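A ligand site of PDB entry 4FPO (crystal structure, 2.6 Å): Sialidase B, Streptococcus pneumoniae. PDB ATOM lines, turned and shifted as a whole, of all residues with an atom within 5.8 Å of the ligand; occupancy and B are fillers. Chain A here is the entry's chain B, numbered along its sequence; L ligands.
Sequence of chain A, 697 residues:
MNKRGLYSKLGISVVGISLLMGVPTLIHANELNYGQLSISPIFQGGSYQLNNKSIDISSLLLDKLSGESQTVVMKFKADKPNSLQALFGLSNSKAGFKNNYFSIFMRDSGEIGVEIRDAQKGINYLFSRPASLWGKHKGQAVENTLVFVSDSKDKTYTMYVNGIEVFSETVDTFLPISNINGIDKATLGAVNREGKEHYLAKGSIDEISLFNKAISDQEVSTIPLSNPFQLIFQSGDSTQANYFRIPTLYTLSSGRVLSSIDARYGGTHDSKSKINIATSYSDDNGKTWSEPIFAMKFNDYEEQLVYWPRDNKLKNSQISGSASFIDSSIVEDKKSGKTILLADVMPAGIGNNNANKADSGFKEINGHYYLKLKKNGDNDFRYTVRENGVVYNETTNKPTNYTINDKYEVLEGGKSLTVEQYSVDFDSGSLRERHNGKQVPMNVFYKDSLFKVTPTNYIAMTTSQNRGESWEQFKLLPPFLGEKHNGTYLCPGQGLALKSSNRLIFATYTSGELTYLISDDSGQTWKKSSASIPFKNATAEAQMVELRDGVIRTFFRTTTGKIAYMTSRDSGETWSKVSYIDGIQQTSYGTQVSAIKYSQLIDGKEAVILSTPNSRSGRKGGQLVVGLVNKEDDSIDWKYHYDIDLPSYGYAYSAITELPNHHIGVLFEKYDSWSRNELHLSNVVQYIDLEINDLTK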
ATOM      1  N   ARG A 245      -8.299   0.044 -16.985  1.00  0.00           N
ATOM      2  CA  ARG A 245      -7.687  -0.208 -15.689  1.00  0.00           C
ATOM      3  C   ARG A 245      -6.281   0.386 -15.763  1.00  0.00           C
ATOM      4  O   ARG A 245      -5.797   0.711 -16.853  1.00  0.00           O
ATOM      5  CB  ARG A 245      -7.603  -1.704 -15.398  1.00  0.00           C
ATOM      6  CG  ARG A 245      -8.726  -2.262 -14.527  1.00  0.00           C
ATOM      7  CD  ARG A 245      -8.266  -3.435 -13.650  1.00  0.00           C
ATOM      8  NE  ARG A 245      -7.363  -3.024 -12.590  1.00  0.00           N
ATOM      9  CZ  ARG A 245      -6.810  -3.845 -11.690  1.00  0.00           C
ATOM     10  NH1 ARG A 245      -7.099  -5.151 -11.735  1.00  0.00           N
ATOM     11  NH2 ARG A 245      -5.981  -3.361 -10.773  1.00  0.00           N
ATOM     12  N   ILE A 246      -5.649   0.509 -14.594  1.00  0.00           N
ATOM     13  CA  ILE A 246      -4.291   1.042 -14.455  1.00  0.00           C
ATOM     14  C   ILE A 246      -4.090   2.471 -15.001  1.00  0.00           C
ATOM     15  O   ILE A 246      -3.376   2.663 -15.991  1.00  0.00           O
ATOM     16  CB  ILE A 246      -3.236   0.125 -15.086  1.00  0.00           C
ATOM     17  CG1 ILE A 246      -3.658  -1.348 -15.032  1.00  0.00           C
ATOM     18  CG2 ILE A 246      -1.931   0.306 -14.379  1.00  0.00           C
ATOM     19  CD1 ILE A 246      -3.713  -1.949 -13.625  1.00  0.00           C
ATOM     20  N   ARG A 264      -8.474  -2.311 -22.001  1.00  0.00           N
ATOM     21  CA  ARG A 264      -8.660  -3.754 -21.822  1.00  0.00           C
ATOM     22  C   ARG A 264      -9.914  -4.275 -22.508  1.00  0.00           C
ATOM     23  O   ARG A 264     -11.037  -3.845 -22.230  1.00  0.00           O
ATOM     24  CB  ARG A 264      -8.633  -4.126 -20.324  1.00  0.00           C
ATOM     25  CG  ARG A 264      -7.347  -3.684 -19.607  1.00  0.00           C
ATOM     26  CD  ARG A 264      -7.315  -4.135 -18.169  1.00  0.00           C
ATOM     27  NE  ARG A 264      -5.956  -4.209 -17.645  1.00  0.00           N
ATOM     28  CZ  ARG A 264      -5.610  -4.796 -16.497  1.00  0.00           C
ATOM     29  NH1 ARG A 264      -6.512  -5.381 -15.719  1.00  0.00           N
ATOM     30  NH2 ARG A 264      -4.345  -4.806 -16.117  1.00  0.00           N
ATOM     31  N   ASP A 270      -6.368  -9.126 -16.021  1.00  0.00           N
ATOM     32  CA  ASP A 270      -4.948  -8.894 -16.320  1.00  0.00           C
ATOM     33  C   ASP A 270      -4.490  -9.737 -17.502  1.00  0.00           C
ATOM     34  O   ASP A 270      -3.812  -9.258 -18.418  1.00  0.00           O
ATOM     35  CB  ASP A 270      -4.085  -9.309 -15.124  1.00  0.00           C
ATOM     36  CG  ASP A 270      -3.988  -8.245 -14.068  1.00  0.00           C
ATOM     37  OD1 ASP A 270      -4.665  -7.202 -14.182  1.00  0.00           O
ATOM     38  OD2 ASP A 270      -3.213  -8.475 -13.109  1.00  0.00           O
ATOM     39  N   SER A 271      -4.868 -11.009 -17.446  1.00  0.00           N
ATOM     40  CA  SER A 271      -4.344 -12.055 -18.305  1.00  0.00           C
ATOM     41  C   SER A 271      -5.236 -13.295 -18.106  1.00  0.00           C
ATOM     42  O   SER A 271      -5.799 -13.483 -17.020  1.00  0.00           O
ATOM     43  CB  SER A 271      -2.905 -12.378 -17.901  1.00  0.00           C
ATOM     44  OG  SER A 271      -2.289 -13.294 -18.787  1.00  0.00           O
ATOM     45  N   ILE A 326       0.336  -4.341 -20.578  1.00  0.00           N
ATOM     46  CA  ILE A 326      -0.283  -4.157 -19.260  1.00  0.00           C
ATOM     47  C   ILE A 326       0.694  -3.318 -18.449  1.00  0.00           C
ATOM     48  O   ILE A 326       1.891  -3.512 -18.561  1.00  0.00           O
ATOM     49  CB  ILE A 326      -0.620  -5.521 -18.550  1.00  0.00           C
ATOM     50  CG1 ILE A 326      -1.263  -5.316 -17.179  1.00  0.00           C
ATOM     51  CG2 ILE A 326       0.597  -6.434 -18.395  1.00  0.00           C
ATOM     52  CD1 ILE A 326      -1.742  -6.632 -16.592  1.00  0.00           C
ATOM     53  N   ASP A 327       0.167  -2.378 -17.661  1.00  0.00           N
ATOM     54  CA  ASP A 327       0.979  -1.519 -16.775  1.00  0.00           C
ATOM     55  C   ASP A 327       1.842  -0.484 -17.537  1.00  0.00           C
ATOM     56  O   ASP A 327       2.945  -0.772 -17.962  1.00  0.00           O
ATOM     57  CB  ASP A 327       1.860  -2.342 -15.825  1.00  0.00           C
ATOM     58  CG  ASP A 327       1.062  -3.126 -14.787  1.00  0.00           C
ATOM     59  OD1 ASP A 327      -0.158  -2.901 -14.665  1.00  0.00           O
ATOM     60  OD2 ASP A 327       1.669  -3.984 -14.090  1.00  0.00           O
ATOM     61  N   ASP A 344       4.738  -3.179 -19.660  1.00  0.00           N
ATOM     62  CA  ASP A 344       5.006  -4.618 -19.744  1.00  0.00           C
ATOM     63  C   ASP A 344       4.419  -5.138 -21.063  1.00  0.00           C
ATOM     64  O   ASP A 344       3.331  -4.708 -21.461  1.00  0.00           O
ATOM     65  CB  ASP A 344       4.380  -5.370 -18.574  1.00  0.00           C
ATOM     66  CG  ASP A 344       4.974  -5.002 -17.214  1.00  0.00           C
ATOM     67  OD1 ASP A 344       6.184  -4.717 -17.113  1.00  0.00           O
ATOM     68  OD2 ASP A 344       4.220  -5.036 -16.218  1.00  0.00           O
ATOM     69  N   VAL A 345       5.135  -6.039 -21.743  1.00  0.00           N
ATOM     70  CA  VAL A 345       4.627  -6.726 -22.944  1.00  0.00           C
ATOM     71  C   VAL A 345       4.608  -8.235 -22.731  1.00  0.00           C
ATOM     72  O   VAL A 345       5.508  -8.790 -22.108  1.00  0.00           O
ATOM     73  CB  VAL A 345       5.561  -6.585 -24.180  1.00  0.00           C
ATOM     74  CG1 VAL A 345       4.724  -6.397 -25.450  1.00  0.00           C
ATOM     75  CG2 VAL A 345       6.584  -5.512 -23.989  1.00  0.00           C
ATOM     76  N   MET A 346       3.608  -8.876 -23.330  1.00  0.00           N
ATOM     77  CA  MET A 346       3.506 -10.336 -23.308  1.00  0.00           C
ATOM     78  C   MET A 346       3.123 -10.833 -24.694  1.00  0.00           C
ATOM     79  O   MET A 346       2.243 -10.266 -25.354  1.00  0.00           O
ATOM     80  CB  MET A 346       2.451 -10.797 -22.299  1.00  0.00           C
ATOM     81  CG  MET A 346       2.760 -10.396 -20.877  1.00  0.00           C
ATOM     82  SD  MET A 346       1.535 -10.957 -19.700  1.00  0.00           S
ATOM     83  CE  MET A 346       0.157  -9.850 -20.055  1.00  0.00           C
ATOM     84  N   ASN A 457       7.412 -12.443 -19.892  1.00  0.00           N
ATOM     85  CA  ASN A 457       7.213 -11.001 -19.910  1.00  0.00           C
ATOM     86  C   ASN A 457       8.475 -10.166 -20.242  1.00  0.00           C
ATOM     87  O   ASN A 457       9.586 -10.479 -19.810  1.00  0.00           O
ATOM     88  CB  ASN A 457       6.596 -10.525 -18.582  1.00  0.00           C
ATOM     89  CG  ASN A 457       7.528 -10.705 -17.398  1.00  0.00           C
ATOM     90  OD1 ASN A 457       8.086 -11.782 -17.189  1.00  0.00           O
ATOM     91  ND2 ASN A 457       7.724  -9.642 -16.635  1.00  0.00           N
ATOM     92  N   TYR A 489       8.923  -6.408 -13.374  1.00  0.00           N
ATOM     93  CA  TYR A 489       7.602  -5.863 -13.627  1.00  0.00           C
ATOM     94  C   TYR A 489       7.580  -4.347 -13.453  1.00  0.00           C
ATOM     95  O   TYR A 489       7.893  -3.839 -12.387  1.00  0.00           O
ATOM     96  CB  TYR A 489       6.585  -6.506 -12.692  1.00  0.00           C
ATOM     97  CG  TYR A 489       6.441  -7.989 -12.940  1.00  0.00           C
ATOM     98  CD1 TYR A 489       5.619  -8.459 -13.957  1.00  0.00           C
ATOM     99  CD2 TYR A 489       7.131  -8.914 -12.170  1.00  0.00           C
ATOM    100  CE1 TYR A 489       5.484  -9.790 -14.196  1.00  0.00           C
ATOM    101  CE2 TYR A 489       7.005 -10.253 -12.401  1.00  0.00           C
ATOM    102  CZ  TYR A 489       6.174 -10.701 -13.423  1.00  0.00           C
ATOM    103  OH  TYR A 489       6.040 -12.046 -13.664  1.00  0.00           O
ATOM    104  N   TYR A 509       9.584  -4.064 -10.248  1.00  0.00           N
ATOM    105  CA  TYR A 509       9.670  -5.018  -9.157  1.00  0.00           C
ATOM    106  C   TYR A 509       9.847  -6.447  -9.636  1.00  0.00           C
ATOM    107  O   TYR A 509       9.347  -6.851 -10.692  1.00  0.00           O
ATOM    108  CB  TYR A 509       8.456  -4.903  -8.212  1.00  0.00           C
ATOM    109  CG  TYR A 509       7.140  -5.326  -8.817  1.00  0.00           C
ATOM    110  CD1 TYR A 509       6.673  -6.629  -8.696  1.00  0.00           C
ATOM    111  CD2 TYR A 509       6.343  -4.404  -9.495  1.00  0.00           C
ATOM    112  CE1 TYR A 509       5.453  -7.007  -9.232  1.00  0.00           C
ATOM    113  CE2 TYR A 509       5.125  -4.773 -10.035  1.00  0.00           C
ATOM    114  CZ  TYR A 509       4.686  -6.077  -9.906  1.00  0.00           C
ATOM    115  OH  TYR A 509       3.472  -6.442 -10.459  1.00  0.00           O
ATOM    116  N   THR A 539       3.620  -8.054  -5.118  1.00  0.00           N
ATOM    117  CA  THR A 539       3.368  -7.099  -6.170  1.00  0.00           C
ATOM    118  C   THR A 539       3.793  -5.742  -5.624  1.00  0.00           C
ATOM    119  O   THR A 539       2.956  -4.929  -5.232  1.00  0.00           O
ATOM    120  CB  THR A 539       1.878  -7.092  -6.559  1.00  0.00           C
ATOM    121  OG1 THR A 539       1.445  -8.450  -6.765  1.00  0.00           O
ATOM    122  CG2 THR A 539       1.653  -6.295  -7.833  1.00  0.00           C
ATOM    123  N   GLU A 541       4.450  -2.788  -6.350  1.00  0.00           N
ATOM    124  CA  GLU A 541       4.205  -1.590  -7.138  1.00  0.00           C
ATOM    125  C   GLU A 541       4.657  -0.349  -6.352  1.00  0.00           C
ATOM    126  O   GLU A 541       4.214  -0.101  -5.226  1.00  0.00           O
ATOM    127  CB  GLU A 541       2.709  -1.510  -7.500  1.00  0.00           C
ATOM    128  CG  GLU A 541       2.289  -2.555  -8.509  1.00  0.00           C
ATOM    129  CD  GLU A 541       0.806  -2.880  -8.445  1.00  0.00           C
ATOM    130  OE1 GLU A 541       0.253  -3.370  -9.464  1.00  0.00           O
ATOM    131  OE2 GLU A 541       0.206  -2.629  -7.385  1.00  0.00           O
ATOM    132  N   ARG A 557       3.606  -0.794  -2.419  1.00  0.00           N
ATOM    133  CA  ARG A 557       2.674  -1.830  -1.980  1.00  0.00           C
ATOM    134  C   ARG A 557       3.355  -3.098  -1.429  1.00  0.00           C
ATOM    135  O   ARG A 557       4.369  -3.554  -1.957  1.00  0.00           O
ATOM    136  CB  ARG A 557       1.786  -2.198  -3.169  1.00  0.00           C
ATOM    137  CG  ARG A 557       0.970  -3.455  -3.023  1.00  0.00           C
ATOM    138  CD  ARG A 557       0.280  -3.756  -4.328  1.00  0.00           C
ATOM    139  NE  ARG A 557      -0.412  -5.039  -4.301  1.00  0.00           N
ATOM    140  CZ  ARG A 557      -1.313  -5.404  -5.210  1.00  0.00           C
ATOM    141  NH1 ARG A 557      -1.603  -4.571  -6.202  1.00  0.00           N
ATOM    142  NH2 ARG A 557      -1.916  -6.575  -5.118  1.00  0.00           N
ATOM    143  N   TYR A 589      -3.284  -8.367   0.420  1.00  0.00           N
ATOM    144  CA  TYR A 589      -2.781  -8.439  -0.958  1.00  0.00           C
ATOM    145  C   TYR A 589      -2.389  -7.056  -1.487  1.00  0.00           C
ATOM    146  O   TYR A 589      -1.554  -6.931  -2.396  1.00  0.00           O
ATOM    147  CB  TYR A 589      -3.788  -9.138  -1.880  1.00  0.00           C
ATOM    148  CG  TYR A 589      -5.159  -8.526  -1.830  1.00  0.00           C
ATOM    149  CD1 TYR A 589      -5.474  -7.406  -2.591  1.00  0.00           C
ATOM    150  CD2 TYR A 589      -6.141  -9.048  -0.979  1.00  0.00           C
ATOM    151  CE1 TYR A 589      -6.713  -6.833  -2.532  1.00  0.00           C
ATOM    152  CE2 TYR A 589      -7.391  -8.470  -0.913  1.00  0.00           C
ATOM    153  CZ  TYR A 589      -7.669  -7.370  -1.701  1.00  0.00           C
ATOM    154  OH  TYR A 589      -8.906  -6.788  -1.646  1.00  0.00           O
ATOM    155  N   GLY A 590      -2.994  -6.018  -0.904  1.00  0.00           N
ATOM    156  CA  GLY A 590      -2.590  -4.646  -1.129  1.00  0.00           C
ATOM    157  C   GLY A 590      -3.062  -4.026  -2.424  1.00  0.00           C
ATOM    158  O   GLY A 590      -3.654  -4.692  -3.269  1.00  0.00           O
ATOM    159  N   ARG A 619     -10.812  -2.766  -1.438  1.00  0.00           N
ATOM    160  CA  ARG A 619     -10.311  -1.593  -2.114  1.00  0.00           C
ATOM    161  C   ARG A 619     -11.405  -0.539  -2.140  1.00  0.00           C
ATOM    162  O   ARG A 619     -12.121  -0.357  -3.128  1.00  0.00           O
ATOM    163  CB  ARG A 619      -9.818  -1.961  -3.513  1.00  0.00           C
ATOM    164  CG  ARG A 619      -8.562  -2.821  -3.462  1.00  0.00           C
ATOM    165  CD  ARG A 619      -8.221  -3.389  -4.809  1.00  0.00           C
ATOM    166  NE  ARG A 619      -6.824  -3.802  -4.908  1.00  0.00           N
ATOM    167  CZ  ARG A 619      -6.267  -4.286  -6.011  1.00  0.00           C
ATOM    168  NH1 ARG A 619      -6.998  -4.417  -7.117  1.00  0.00           N
ATOM    169  NH2 ARG A 619      -4.986  -4.634  -6.023  1.00  0.00           N
ATOM    170  N   TYR A 653      -6.612   1.275  -7.941  1.00  0.00           N
ATOM    171  CA  TYR A 653      -5.433   1.882  -8.553  1.00  0.00           C
ATOM    172  C   TYR A 653      -5.735   3.343  -8.845  1.00  0.00           C
ATOM    173  O   TYR A 653      -6.865   3.686  -9.205  1.00  0.00           O
ATOM    174  CB  TYR A 653      -5.057   1.154  -9.846  1.00  0.00           C
ATOM    175  CG  TYR A 653      -4.254  -0.122  -9.637  1.00  0.00           C
ATOM    176  CD1 TYR A 653      -4.700  -1.110  -8.770  1.00  0.00           C
ATOM    177  CD2 TYR A 653      -3.057  -0.329 -10.332  1.00  0.00           C
ATOM    178  CE1 TYR A 653      -3.972  -2.282  -8.581  1.00  0.00           C
ATOM    179  CE2 TYR A 653      -2.326  -1.497 -10.157  1.00  0.00           C
ATOM    180  CZ  TYR A 653      -2.795  -2.475  -9.277  1.00  0.00           C
ATOM    181  OH  TYR A 653      -2.078  -3.633  -9.088  1.00  0.00           O
ATOM    182  N   SER A 673     -11.361  -3.385  -7.775  1.00  0.00           N
ATOM    183  CA  SER A 673     -10.798  -4.108  -8.916  1.00  0.00           C
ATOM    184  C   SER A 673     -10.116  -5.408  -8.488  1.00  0.00           C
ATOM    185  O   SER A 673      -9.417  -6.058  -9.281  1.00  0.00           O
ATOM    186  CB  SER A 673      -9.828  -3.216  -9.699  1.00  0.00           C
ATOM    187  OG  SER A 673      -8.691  -2.862  -8.935  1.00  0.00           O
ATOM    188  N   TRP A 674     -10.316  -5.787  -7.222  1.00  0.00           N
ATOM    189  CA  TRP A 674      -9.858  -7.088  -6.733  1.00  0.00           C
ATOM    190  C   TRP A 674     -11.031  -8.068  -6.626  1.00  0.00           C
ATOM    191  O   TRP A 674     -10.936  -9.216  -7.052  1.00  0.00           O
ATOM    192  CB  TRP A 674      -9.150  -6.937  -5.384  1.00  0.00           C
ATOM    193  CG  TRP A 674      -8.570  -8.205  -4.883  1.00  0.00           C
ATOM    194  CD1 TRP A 674      -9.183  -9.133  -4.081  1.00  0.00           C
ATOM    195  CD2 TRP A 674      -7.253  -8.721  -5.155  1.00  0.00           C
ATOM    196  NE1 TRP A 674      -8.331 -10.185  -3.846  1.00  0.00           N
ATOM    197  CE2 TRP A 674      -7.142  -9.960  -4.484  1.00  0.00           C
ATOM    198  CE3 TRP A 674      -6.153  -8.256  -5.907  1.00  0.00           C
ATOM    199  CZ2 TRP A 674      -5.982 -10.746  -4.536  1.00  0.00           C
ATOM    200  CZ3 TRP A 674      -5.007  -9.032  -5.945  1.00  0.00           C
ATOM    201  CH2 TRP A 674      -4.929 -10.261  -5.265  1.00  0.00           C
HETATM  202  O1  LIG L   1      -4.482  -7.997  -9.231  1.00  0.00           O
HETATM  203  S1  LIG L   1      -4.238  -6.585  -9.129  1.00  0.00           S
HETATM  204  O2  LIG L   1      -3.430  -6.249  -7.872  1.00  0.00           O
HETATM  205  O3  LIG L   1      -5.505  -5.859  -9.070  1.00  0.00           O
HETATM  206  C1  LIG L   1      -3.282  -6.132 -10.503  1.00  0.00           C
HETATM  207  C2  LIG L   1      -1.870  -6.777 -10.559  1.00  0.00           C
HETATM  208  N1  LIG L   1      -1.302  -6.942 -11.878  1.00  0.00           N
HETATM  209  C3  LIG L   1      -0.146  -7.866 -11.804  1.00  0.00           C
HETATM  210  C4  LIG L   1       0.448  -8.205 -13.075  1.00  0.00           C
HETATM  211  C5  LIG L   1      -0.142  -9.201 -13.872  1.00  0.00           C
HETATM  212  C6  LIG L   1       0.411  -9.537 -15.108  1.00  0.00           C
HETATM  213 CL1  LIG L   1      -0.312 -10.765 -16.079  1.00  0.00          CL
HETATM  214  C7  LIG L   1       1.588  -8.866 -15.557  1.00  0.00           C
HETATM  215  O4  LIG L   1       2.164  -9.199 -16.801  1.00  0.00           O
HETATM  216  C8  LIG L   1       3.400  -8.693 -17.092  1.00  0.00           C
HETATM  217  C9  LIG L   1       2.154  -7.893 -14.789  1.00  0.00           C
HETATM  218  C10 LIG L   1       1.579  -7.541 -13.508  1.00  0.00           C
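The side-chain hydroxyl (OG) of Ser 673 lies within hydrogen-bond range of the guanidinium group (NH1) of Arg 619. The guanidinium group of Arg 619 sits at hydrogen-bond distance from the backbone carbonyl oxygen of Gly 590 (3.1 Å). NH1 of Arg 557 lies within salt-bridge range of OE2 of Glu 541 (2.9 Å). NH2 of Arg 557 sits at hydrogen-bond distance from O of Tyr 589, 2.8 Å away. The side-chain hydroxyl (OG) of Ser 673 sits at hydrogen-bond distance from the guanidinium group (NH2) of Arg 245, 3.3 Å away. OE2 of Glu 541 lies within hydrogen-bond range of OH of Tyr 653 (3.0 Å). N of Asp 344 lies within hydrogen-bond range of O of Ile 326, 3.1 Å away. The backbone carbonyl oxygen (O) of Asp 327 lies within hydrogen-bond range of the backbone NH (N) of Asp 344.
The side-chain carboxylate of Asp 270 lies within salt-bridge range of a nitrogen (N1) of the ligand, at 2.7 Å. NH1 of Arg 619 is in salt-bridge range of O3 of the ligand, at 2.9 Å. An oxygen (O2) of the ligand lies within salt-bridge range of the guanidinium group of Arg 557. NH2 of Arg 245 lies within salt-bridge range of O3 of the ligand, 3.1 Å away. An oxygen (O2) of the ligand sits close to the side-chain hydroxyl (OH) of Tyr 653 (3.2 Å).
SD of Met 346 lies close to O4 of the ligand, at 3.4 Å. Residues that only touch the ligand: Ser 271, Ile 326, Asp 327, Asp 344, Asn 457, Tyr 489, Tyr 509, Ser 673 and Trp 674. Hydrophobic or aromatic side chains within 4 Å of the ligand: Ile 326, Met 346, Tyr 489, Tyr 653 and Trp 674. Of the 22 residues printed, 15 come within 4 Å of the ligand.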
